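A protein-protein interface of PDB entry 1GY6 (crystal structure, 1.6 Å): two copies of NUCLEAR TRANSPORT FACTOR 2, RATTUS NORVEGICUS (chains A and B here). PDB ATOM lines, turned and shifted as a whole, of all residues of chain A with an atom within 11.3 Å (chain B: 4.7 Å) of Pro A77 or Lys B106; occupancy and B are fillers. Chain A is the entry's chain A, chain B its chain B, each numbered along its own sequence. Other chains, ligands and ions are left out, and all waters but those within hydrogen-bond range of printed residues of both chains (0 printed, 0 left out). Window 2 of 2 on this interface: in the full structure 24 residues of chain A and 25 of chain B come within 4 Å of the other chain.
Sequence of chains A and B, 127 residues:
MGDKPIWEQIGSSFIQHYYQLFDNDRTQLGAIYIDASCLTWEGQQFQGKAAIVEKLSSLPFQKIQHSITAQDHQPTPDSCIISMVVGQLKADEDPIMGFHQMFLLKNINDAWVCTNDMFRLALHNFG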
ATOM      1  N   TRP A   7      11.141  18.378  -4.579  1.00  0.00           N
ATOM      2  CA  TRP A   7      10.433  19.475  -3.936  1.00  0.00           C
ATOM      3  C   TRP A   7      10.090  20.588  -4.885  1.00  0.00           C
ATOM      4  O   TRP A   7       9.075  21.251  -4.691  1.00  0.00           O
ATOM      5  CB  TRP A   7      11.194  20.041  -2.726  1.00  0.00           C
ATOM      6  CG  TRP A   7      12.660  20.312  -2.947  1.00  0.00           C
ATOM      7  CD1 TRP A   7      13.240  21.463  -3.386  1.00  0.00           C
ATOM      8  CD2 TRP A   7      13.730  19.386  -2.714  1.00  0.00           C
ATOM      9  NE1 TRP A   7      14.611  21.312  -3.445  1.00  0.00           N
ATOM     10  CE2 TRP A   7      14.931  20.043  -3.043  1.00  0.00           C
ATOM     11  CE3 TRP A   7      13.778  18.063  -2.268  1.00  0.00           C
ATOM     12  CZ2 TRP A   7      16.186  19.409  -2.938  1.00  0.00           C
ATOM     13  CZ3 TRP A   7      15.035  17.427  -2.162  1.00  0.00           C
ATOM     14  CH2 TRP A   7      16.203  18.115  -2.502  1.00  0.00           C
ATOM     15  N   HIS A  73      11.270  26.908  -3.671  1.00  0.00           N
ATOM     16  CA  HIS A  73      10.878  25.735  -2.903  1.00  0.00           C
ATOM     17  C   HIS A  73      12.083  25.083  -2.223  1.00  0.00           C
ATOM     18  O   HIS A  73      13.191  25.086  -2.766  1.00  0.00           O
ATOM     19  CB  HIS A  73      10.245  24.688  -3.825  1.00  0.00           C
ATOM     20  CG  HIS A  73       9.105  25.226  -4.625  1.00  0.00           C
ATOM     21  ND1 HIS A  73       9.248  25.712  -5.906  1.00  0.00           N
ATOM     22  CD2 HIS A  73       7.808  25.406  -4.292  1.00  0.00           C
ATOM     23  CE1 HIS A  73       8.079  26.177  -6.326  1.00  0.00           C
ATOM     24  NE2 HIS A  73       7.192  26.003  -5.362  1.00  0.00           N
ATOM     25  N   GLN A  74      11.866  24.545  -1.030  1.00  0.00           N
ATOM     26  CA  GLN A  74      12.939  23.840  -0.321  1.00  0.00           C
ATOM     27  C   GLN A  74      12.341  22.715   0.500  1.00  0.00           C
ATOM     28  O   GLN A  74      11.170  22.795   0.911  1.00  0.00           O
ATOM     29  CB  GLN A  74      13.638  24.759   0.698  1.00  0.00           C
ATOM     30  CG  GLN A  74      14.494  25.877   0.161  1.00  0.00           C
ATOM     31  CD  GLN A  74      14.918  26.820   1.283  1.00  0.00           C
ATOM     32  OE1 GLN A  74      14.558  26.608   2.457  1.00  0.00           O
ATOM     33  NE2 GLN A  74      15.690  27.847   0.955  1.00  0.00           N
ATOM     34  N   PRO A  75      13.137  21.652   0.754  1.00  0.00           N
ATOM     35  CA  PRO A  75      12.683  20.531   1.583  1.00  0.00           C
ATOM     36  C   PRO A  75      12.932  20.971   3.037  1.00  0.00           C
ATOM     37  O   PRO A  75      13.874  21.751   3.311  1.00  0.00           O
ATOM     38  CB  PRO A  75      13.605  19.381   1.174  1.00  0.00           C
ATOM     39  CG  PRO A  75      14.886  20.066   0.775  1.00  0.00           C
ATOM     40  CD  PRO A  75      14.474  21.403   0.168  1.00  0.00           C
ATOM     41  N   THR A  76      12.130  20.475   3.972  1.00  0.00           N
ATOM     42  CA  THR A  76      12.318  20.850   5.387  1.00  0.00           C
ATOM     43  C   THR A  76      12.748  19.619   6.181  1.00  0.00           C
ATOM     44  O   THR A  76      12.577  18.489   5.726  1.00  0.00           O
ATOM     45  CB  THR A  76      11.031  21.402   5.990  1.00  0.00           C
ATOM     46  OG1 THR A  76      10.139  20.304   6.206  1.00  0.00           O
ATOM     47  CG2 THR A  76      10.373  22.418   5.064  1.00  0.00           C
ATOM     48  N   PRO A  77      13.274  19.806   7.408  1.00  0.00           N
ATOM     49  CA  PRO A  77      13.724  18.637   8.197  1.00  0.00           C
ATOM     50  C   PRO A  77      12.708  17.530   8.491  1.00  0.00           C
ATOM     51  O   PRO A  77      13.107  16.383   8.759  1.00  0.00           O
ATOM     52  CB  PRO A  77      14.272  19.280   9.474  1.00  0.00           C
ATOM     53  CG  PRO A  77      14.805  20.603   8.968  1.00  0.00           C
ATOM     54  CD  PRO A  77      13.637  21.064   8.087  1.00  0.00           C
ATOM     55  N   ASP A  78      11.412  17.854   8.467  1.00  0.00           N
ATOM     56  CA  ASP A  78      10.375  16.854   8.750  1.00  0.00           C
ATOM     57  C   ASP A  78       9.717  16.321   7.464  1.00  0.00           C
ATOM     58  O   ASP A  78       8.523  16.009   7.449  1.00  0.00           O
ATOM     59  CB  ASP A  78       9.286  17.455   9.669  1.00  0.00           C
ATOM     60  CG  ASP A  78       9.823  17.865  11.041  1.00  0.00           C
ATOM     61  OD1 ASP A  78      10.278  16.978  11.788  1.00  0.00           O
ATOM     62  OD2 ASP A  78       9.787  19.070  11.375  1.00  0.00           O
ATOM     63  N   SER A  79      10.494  16.225   6.387  1.00  0.00           N
ATOM     64  CA  SER A  79       9.985  15.723   5.112  1.00  0.00           C
ATOM     65  C   SER A  79       8.872  16.557   4.476  1.00  0.00           C
ATOM     66  O   SER A  79       8.087  16.046   3.683  1.00  0.00           O
ATOM     67  CB  SER A  79       9.491  14.279   5.242  1.00  0.00           C
ATOM     68  OG  SER A  79      10.588  13.412   5.478  1.00  0.00           O
ATOM     69  N   CYS A  80       8.780  17.834   4.831  1.00  0.00           N
ATOM     70  CA  CYS A  80       7.782  18.662   4.187  1.00  0.00           C
ATOM     71  C   CYS A  80       8.435  19.500   3.078  1.00  0.00           C
ATOM     72  O   CYS A  80       9.659  19.464   2.891  1.00  0.00           O
ATOM     73  CB  CYS A  80       7.105  19.596   5.177  1.00  0.00           C
ATOM     74  SG  CYS A  80       6.014  18.672   6.304  1.00  0.00           S
ATOM     75  N   ILE A  81       7.613  20.246   2.351  1.00  0.00           N
ATOM     76  CA  ILE A  81       8.082  21.156   1.288  1.00  0.00           C
ATOM     77  C   ILE A  81       7.573  22.553   1.615  1.00  0.00           C
ATOM     78  O   ILE A  81       6.364  22.739   1.848  1.00  0.00           O
ATOM     79  CB  ILE A  81       7.546  20.754  -0.099  1.00  0.00           C
ATOM     80  CG1 ILE A  81       8.127  19.396  -0.481  1.00  0.00           C
ATOM     81  CG2 ILE A  81       7.976  21.765  -1.148  1.00  0.00           C
ATOM     82  CD1 ILE A  81       7.457  18.800  -1.721  1.00  0.00           C
ATOM     83  N   ILE A  82       8.477  23.534   1.663  1.00  0.00           N
ATOM     84  CA  ILE A  82       8.056  24.890   1.975  1.00  0.00           C
ATOM     85  C   ILE A  82       8.264  25.715   0.726  1.00  0.00           C
ATOM     86  O   ILE A  82       9.249  25.544   0.002  1.00  0.00           O
ATOM     87  CB  ILE A  82       8.814  25.447   3.208  1.00  0.00           C
ATOM     88  CG1 ILE A  82       8.171  26.757   3.664  1.00  0.00           C
ATOM     89  CG2 ILE A  82      10.290  25.589   2.915  1.00  0.00           C
ATOM     90  CD1 ILE A  82       8.507  27.060   5.122  1.00  0.00           C
ATOM     91  N   LEU A 104       3.160  25.427   3.162  1.00  0.00           N
ATOM     92  CA  LEU A 104       3.923  24.288   3.719  1.00  0.00           C
ATOM     93  C   LEU A 104       3.127  23.057   3.302  1.00  0.00           C
ATOM     94  O   LEU A 104       1.924  22.952   3.593  1.00  0.00           O
ATOM     95  CB  LEU A 104       4.028  24.360   5.232  1.00  0.00           C
ATOM     96  CG  LEU A 104       4.865  23.244   5.859  1.00  0.00           C
ATOM     97  CD1 LEU A 104       6.314  23.294   5.323  1.00  0.00           C
ATOM     98  CD2 LEU A 104       4.832  23.395   7.368  1.00  0.00           C
ATOM     99  N   LEU A 105       3.772  22.131   2.594  1.00  0.00           N
ATOM    100  CA  LEU A 105       3.095  20.931   2.119  1.00  0.00           C
ATOM    101  C   LEU A 105       3.619  19.675   2.812  1.00  0.00           C
ATOM    102  O   LEU A 105       4.822  19.556   3.081  1.00  0.00           O
ATOM    103  CB  LEU A 105       3.336  20.773   0.622  1.00  0.00           C
ATOM    104  CG  LEU A 105       3.086  22.034  -0.208  1.00  0.00           C
ATOM    105  CD1 LEU A 105       3.413  21.714  -1.670  1.00  0.00           C
ATOM    106  CD2 LEU A 105       1.634  22.525  -0.028  1.00  0.00           C
ATOM    107  N   LYS A 106       2.721  18.741   3.091  1.00  0.00           N
ATOM    108  CA  LYS A 106       3.110  17.495   3.738  1.00  0.00           C
ATOM    109  C   LYS A 106       2.456  16.367   2.943  1.00  0.00           C
ATOM    110  O   LYS A 106       1.351  16.517   2.429  1.00  0.00           O
ATOM    111  CB  LYS A 106       2.594  17.479   5.161  1.00  0.00           C
ATOM    112  CG  LYS A 106       2.994  16.264   5.985  1.00  0.00           C
ATOM    113  CD  LYS A 106       2.495  16.431   7.409  1.00  0.00           C
ATOM    114  CE  LYS A 106       3.087  17.666   8.078  1.00  0.00           C
ATOM    115  NZ  LYS A 106       2.509  18.037   9.427  1.00  0.00           N
ATOM    116  N   TRP A 112       0.121  15.189  -1.617  1.00  0.00           N
ATOM    117  CA  TRP A 112       0.687  16.375  -0.975  1.00  0.00           C
ATOM    118  C   TRP A 112      -0.436  17.361  -0.714  1.00  0.00           C
ATOM    119  O   TRP A 112      -1.148  17.756  -1.640  1.00  0.00           O
ATOM    120  CB  TRP A 112       1.746  17.028  -1.872  1.00  0.00           C
ATOM    121  CG  TRP A 112       3.019  16.239  -1.930  1.00  0.00           C
ATOM    122  CD1 TRP A 112       3.377  15.305  -2.881  1.00  0.00           C
ATOM    123  CD2 TRP A 112       4.093  16.278  -0.986  1.00  0.00           C
ATOM    124  NE1 TRP A 112       4.602  14.770  -2.578  1.00  0.00           N
ATOM    125  CE2 TRP A 112       5.067  15.347  -1.421  1.00  0.00           C
ATOM    126  CE3 TRP A 112       4.332  17.010   0.183  1.00  0.00           C
ATOM    127  CZ2 TRP A 112       6.256  15.131  -0.725  1.00  0.00           C
ATOM    128  CZ3 TRP A 112       5.522  16.792   0.878  1.00  0.00           C
ATOM    129  CH2 TRP A 112       6.465  15.862   0.422  1.00  0.00           C
ATOM    130  N   CYS B  80       6.937  23.359  14.468  1.00  0.00           N
ATOM    131  CA  CYS B  80       7.779  24.401  13.902  1.00  0.00           C
ATOM    132  C   CYS B  80       6.966  25.690  13.825  1.00  0.00           C
ATOM    133  O   CYS B  80       5.769  25.714  14.158  1.00  0.00           O
ATOM    134  CB  CYS B  80       8.260  24.032  12.491  1.00  0.00           C
ATOM    135  SG  CYS B  80       9.387  22.609  12.515  1.00  0.00           S
ATOM    136  N   LEU B 104      11.632  29.342   8.380  1.00  0.00           N
ATOM    137  CA  LEU B 104      10.998  28.213   9.054  1.00  0.00           C
ATOM    138  C   LEU B 104      11.904  27.969  10.257  1.00  0.00           C
ATOM    139  O   LEU B 104      13.134  27.846  10.109  1.00  0.00           O
ATOM    140  CB  LEU B 104      10.946  26.969   8.158  1.00  0.00           C
ATOM    141  CG  LEU B 104      10.288  25.762   8.832  1.00  0.00           C
ATOM    142  CD1 LEU B 104       8.806  26.009   9.100  1.00  0.00           C
ATOM    143  CD2 LEU B 104      10.462  24.562   7.900  1.00  0.00           C
ATOM    144  N   LEU B 105      11.298  27.931  11.447  1.00  0.00           N
ATOM    145  CA  LEU B 105      12.028  27.766  12.717  1.00  0.00           C
ATOM    146  C   LEU B 105      11.668  26.454  13.399  1.00  0.00           C
ATOM    147  O   LEU B 105      10.526  25.991  13.311  1.00  0.00           O
ATOM    148  CB  LEU B 105      11.648  28.902  13.659  1.00  0.00           C
ATOM    149  CG  LEU B 105      11.655  30.309  13.034  1.00  0.00           C
ATOM    150  CD1 LEU B 105      11.166  31.279  14.101  1.00  0.00           C
ATOM    151  CD2 LEU B 105      13.051  30.683  12.506  1.00  0.00           C
ATOM    152  N   LYS B 106      12.644  25.875  14.093  1.00  0.00           N
ATOM    153  CA  LYS B 106      12.445  24.613  14.800  1.00  0.00           C
ATOM    154  C   LYS B 106      13.220  24.703  16.094  1.00  0.00           C
ATOM    155  O   LYS B 106      14.235  25.382  16.169  1.00  0.00           O
ATOM    156  CB  LYS B 106      12.994  23.444  13.963  1.00  0.00           C
ATOM    157  CG  LYS B 106      12.742  22.046  14.550  1.00  0.00           C
ATOM    158  CD  LYS B 106      13.048  20.969  13.519  1.00  0.00           C
ATOM    159  CE  LYS B 106      13.253  19.625  14.207  1.00  0.00           C
ATOM    160  NZ  LYS B 106      13.776  18.598  13.267  1.00  0.00           N
ATOM    161  N   ASN B 107      12.737  24.028  17.136  1.00  0.00           N
ATOM    162  CA  ASN B 107      13.479  24.056  18.376  1.00  0.00           C
ATOM    163  C   ASN B 107      14.381  22.823  18.388  1.00  0.00           C
ATOM    164  O   ASN B 107      13.896  21.689  18.414  1.00  0.00           O
ATOM    165  CB  ASN B 107      12.556  24.025  19.573  1.00  0.00           C
ATOM    166  CG  ASN B 107      13.319  24.240  20.851  1.00  0.00           C
ATOM    167  OD1 ASN B 107      14.141  23.403  21.225  1.00  0.00           O
ATOM    168  ND2 ASN B 107      13.103  25.383  21.497  1.00  0.00           N
ATOM    169  N   ILE B 108      15.684  23.067  18.321  1.00  0.00           N
ATOM    170  CA  ILE B 108      16.685  22.000  18.285  1.00  0.00           C
ATOM    171  C   ILE B 108      17.674  22.270  19.411  1.00  0.00           C
ATOM    172  O   ILE B 108      18.210  23.372  19.519  1.00  0.00           O
ATOM    173  CB  ILE B 108      17.413  21.998  16.918  1.00  0.00           C
ATOM    174  CG1 ILE B 108      16.404  21.713  15.803  1.00  0.00           C
ATOM    175  CG2 ILE B 108      18.516  20.923  16.893  1.00  0.00           C
ATOM    176  CD1 ILE B 108      16.915  22.043  14.406  1.00  0.00           C
ATOM    177  N   ALA B 111      16.505  25.232  21.712  1.00  0.00           N
ATOM    178  CA  ALA B 111      16.671  26.601  21.246  1.00  0.00           C
ATOM    179  C   ALA B 111      16.001  26.745  19.878  1.00  0.00           C
ATOM    180  O   ALA B 111      16.119  25.858  19.047  1.00  0.00           O
ATOM    181  CB  ALA B 111      18.151  26.931  21.145  1.00  0.00           C
ATOM    182  N   TRP B 112      15.292  27.849  19.651  1.00  0.00           N
ATOM    183  CA  TRP B 112      14.651  28.039  18.342  1.00  0.00           C
ATOM    184  C   TRP B 112      15.703  28.538  17.357  1.00  0.00           C
ATOM    185  O   TRP B 112      16.387  29.542  17.628  1.00  0.00           O
ATOM    186  CB  TRP B 112      13.508  29.041  18.460  1.00  0.00           C
ATOM    187  CG  TRP B 112      12.325  28.459  19.111  1.00  0.00           C
ATOM    188  CD1 TRP B 112      12.003  28.508  20.451  1.00  0.00           C
ATOM    189  CD2 TRP B 112      11.317  27.677  18.487  1.00  0.00           C
ATOM    190  NE1 TRP B 112      10.848  27.796  20.681  1.00  0.00           N
ATOM    191  CE2 TRP B 112      10.408  27.273  19.496  1.00  0.00           C
ATOM    192  CE3 TRP B 112      11.085  27.267  17.159  1.00  0.00           C
ATOM    193  CZ2 TRP B 112       9.287  26.482  19.224  1.00  0.00           C
ATOM    194  CZ3 TRP B 112       9.977  26.488  16.882  1.00  0.00           C
ATOM    195  CH2 TRP B 112       9.081  26.096  17.919  1.00  0.00           C
ATOM    196  N   VAL B 113      15.782  27.862  16.203  1.00  0.00           N
ATOM    197  CA  VAL B 113      16.767  28.176  15.171  1.00  0.00           C
ATOM    198  C   VAL B 113      16.102  28.085  13.802  1.00  0.00           C
ATOM    199  O   VAL B 113      15.039  27.468  13.648  1.00  0.00           O
ATOM    200  CB  VAL B 113      17.960  27.189  15.223  1.00  0.00           C
ATOM    201  CG1 VAL B 113      18.652  27.301  16.556  1.00  0.00           C
ATOM    202  CG2 VAL B 113      17.496  25.773  14.993  1.00  0.00           C
ATOM    203  N   THR B 115      15.823  26.749  10.084  1.00  0.00           N
ATOM    204  CA  THR B 115      16.245  25.634   9.214  1.00  0.00           C
ATOM    205  C   THR B 115      16.144  25.993   7.731  1.00  0.00           C
ATOM    206  O   THR B 115      16.860  25.417   6.884  1.00  0.00           O
ATOM    207  CB  THR B 115      15.383  24.371   9.469  1.00  0.00           C
ATOM    208  OG1 THR B 115      13.998  24.644   9.225  1.00  0.00           O
ATOM    209  CG2 THR B 115      15.571  23.902  10.923  1.00  0.00           C
ATOM    210  N   ASN B 116      15.236  26.909   7.404  1.00  0.00           N
ATOM    211  CA  ASN B 116      14.966  27.274   6.015  1.00  0.00           C
ATOM    212  C   ASN B 116      14.718  28.771   5.966  1.00  0.00           C
ATOM    213  O   ASN B 116      13.993  29.318   6.792  1.00  0.00           O
ATOM    214  CB  ASN B 116      13.710  26.547   5.527  1.00  0.00           C
ATOM    215  CG  ASN B 116      13.889  25.057   5.431  1.00  0.00           C
ATOM    216  OD1 ASN B 116      14.176  24.527   4.350  1.00  0.00           O
ATOM    217  ND2 ASN B 116      13.702  24.363   6.529  1.00  0.00           N
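The side-chain amide oxygen of Gln A74 sits close to the side-chain amide oxygen of Asn B116 (2.8 Å). OD1 of Asn B116 sits close to O of Pro A75, 3.0 Å away. OD2 of Asp A78 sits at hydrogen-bond distance from SG of Cys B80 (3.7 Å).
The backbone carbonyl oxygen of Gln A74 lies within hydrogen-bond range of the backbone NH of Ile A82, at 2.9 Å. N of Cys A80 sits at hydrogen-bond distance from OG1 of Thr A76, at 3.1 Å. The backbone carbonyl oxygen (O) of Leu B104 sits at hydrogen-bond distance from the backbone NH (N) of Thr B115 (2.9 Å). O of Asn B116 sits at hydrogen-bond distance from N of Leu B104 (2.8 Å). The backbone carbonyl oxygen of Val B113 is in hydrogen-bond range of the backbone NH of Lys B106, 2.9 Å away. The side-chain hydroxyl (OG1) of Thr B115 lies within hydrogen-bond range of the side-chain amide nitrogen (ND2) of Asn B116 (2.7 Å).
Among the printed residues, pairs that only touch across the chains: Thr A76 with Leu B104, Thr A76 with Asn B116, Pro A77 with Lys B106, Pro A77 with Thr B115, Pro A77 with Asn B116 and Ile A82 with Leu B104.
Pro A77 touches three residues of chain B. Cys B80 touches one residue of chain A. Asn B107 touches none of the printed residues of chain A. No residue of chain A comes within 4 Å of Ile B108. No residue of chain A comes within 4 Å of Ala B111. No residue of chain A comes within 4 Å of Trp B112. No residue of chain A comes within 4 Å of Val B113. Printed residues of chain A within 4 Å of Thr B115: Pro A77. Of the printed residues of chain A, Asn B116 touches Gln A74, Pro A75, Thr A76 and Pro A77. Of the printed residues of chain B, Ile A82 touches Leu B104. Lys A106 touches none of the printed residues of chain B. Trp A112 touches none of the printed residues of chain B. The nearest printed residue of chain B that does not touch Pro A77 is Leu B104 (4.7 Å). The nearest printed residue of chain B that does not touch Ile A82 is Asn B116 (4.3 Å).
Printed residues of chain A that touch a printed residue of chain B: Gln A74, Pro A75, Thr A76, Pro A77, Asp A78 and Ile A82. Hydrophobic or aromatic side chains of chain A that line the printed part of chain B: Pro A77 and Ile A82. Of the 11 printed residues of chain B, 5 touch a printed residue of chain A. Hydrophobic or aromatic side chains of chain B that line the printed part of chain A: Leu B104. Among the printed residues, no Asp or Glu carboxylate lies within 4 Å of a Lys or Arg side-chain nitrogen of the other chain.
Positions printed for both chains: 80, 104, 105, 106 and 112.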
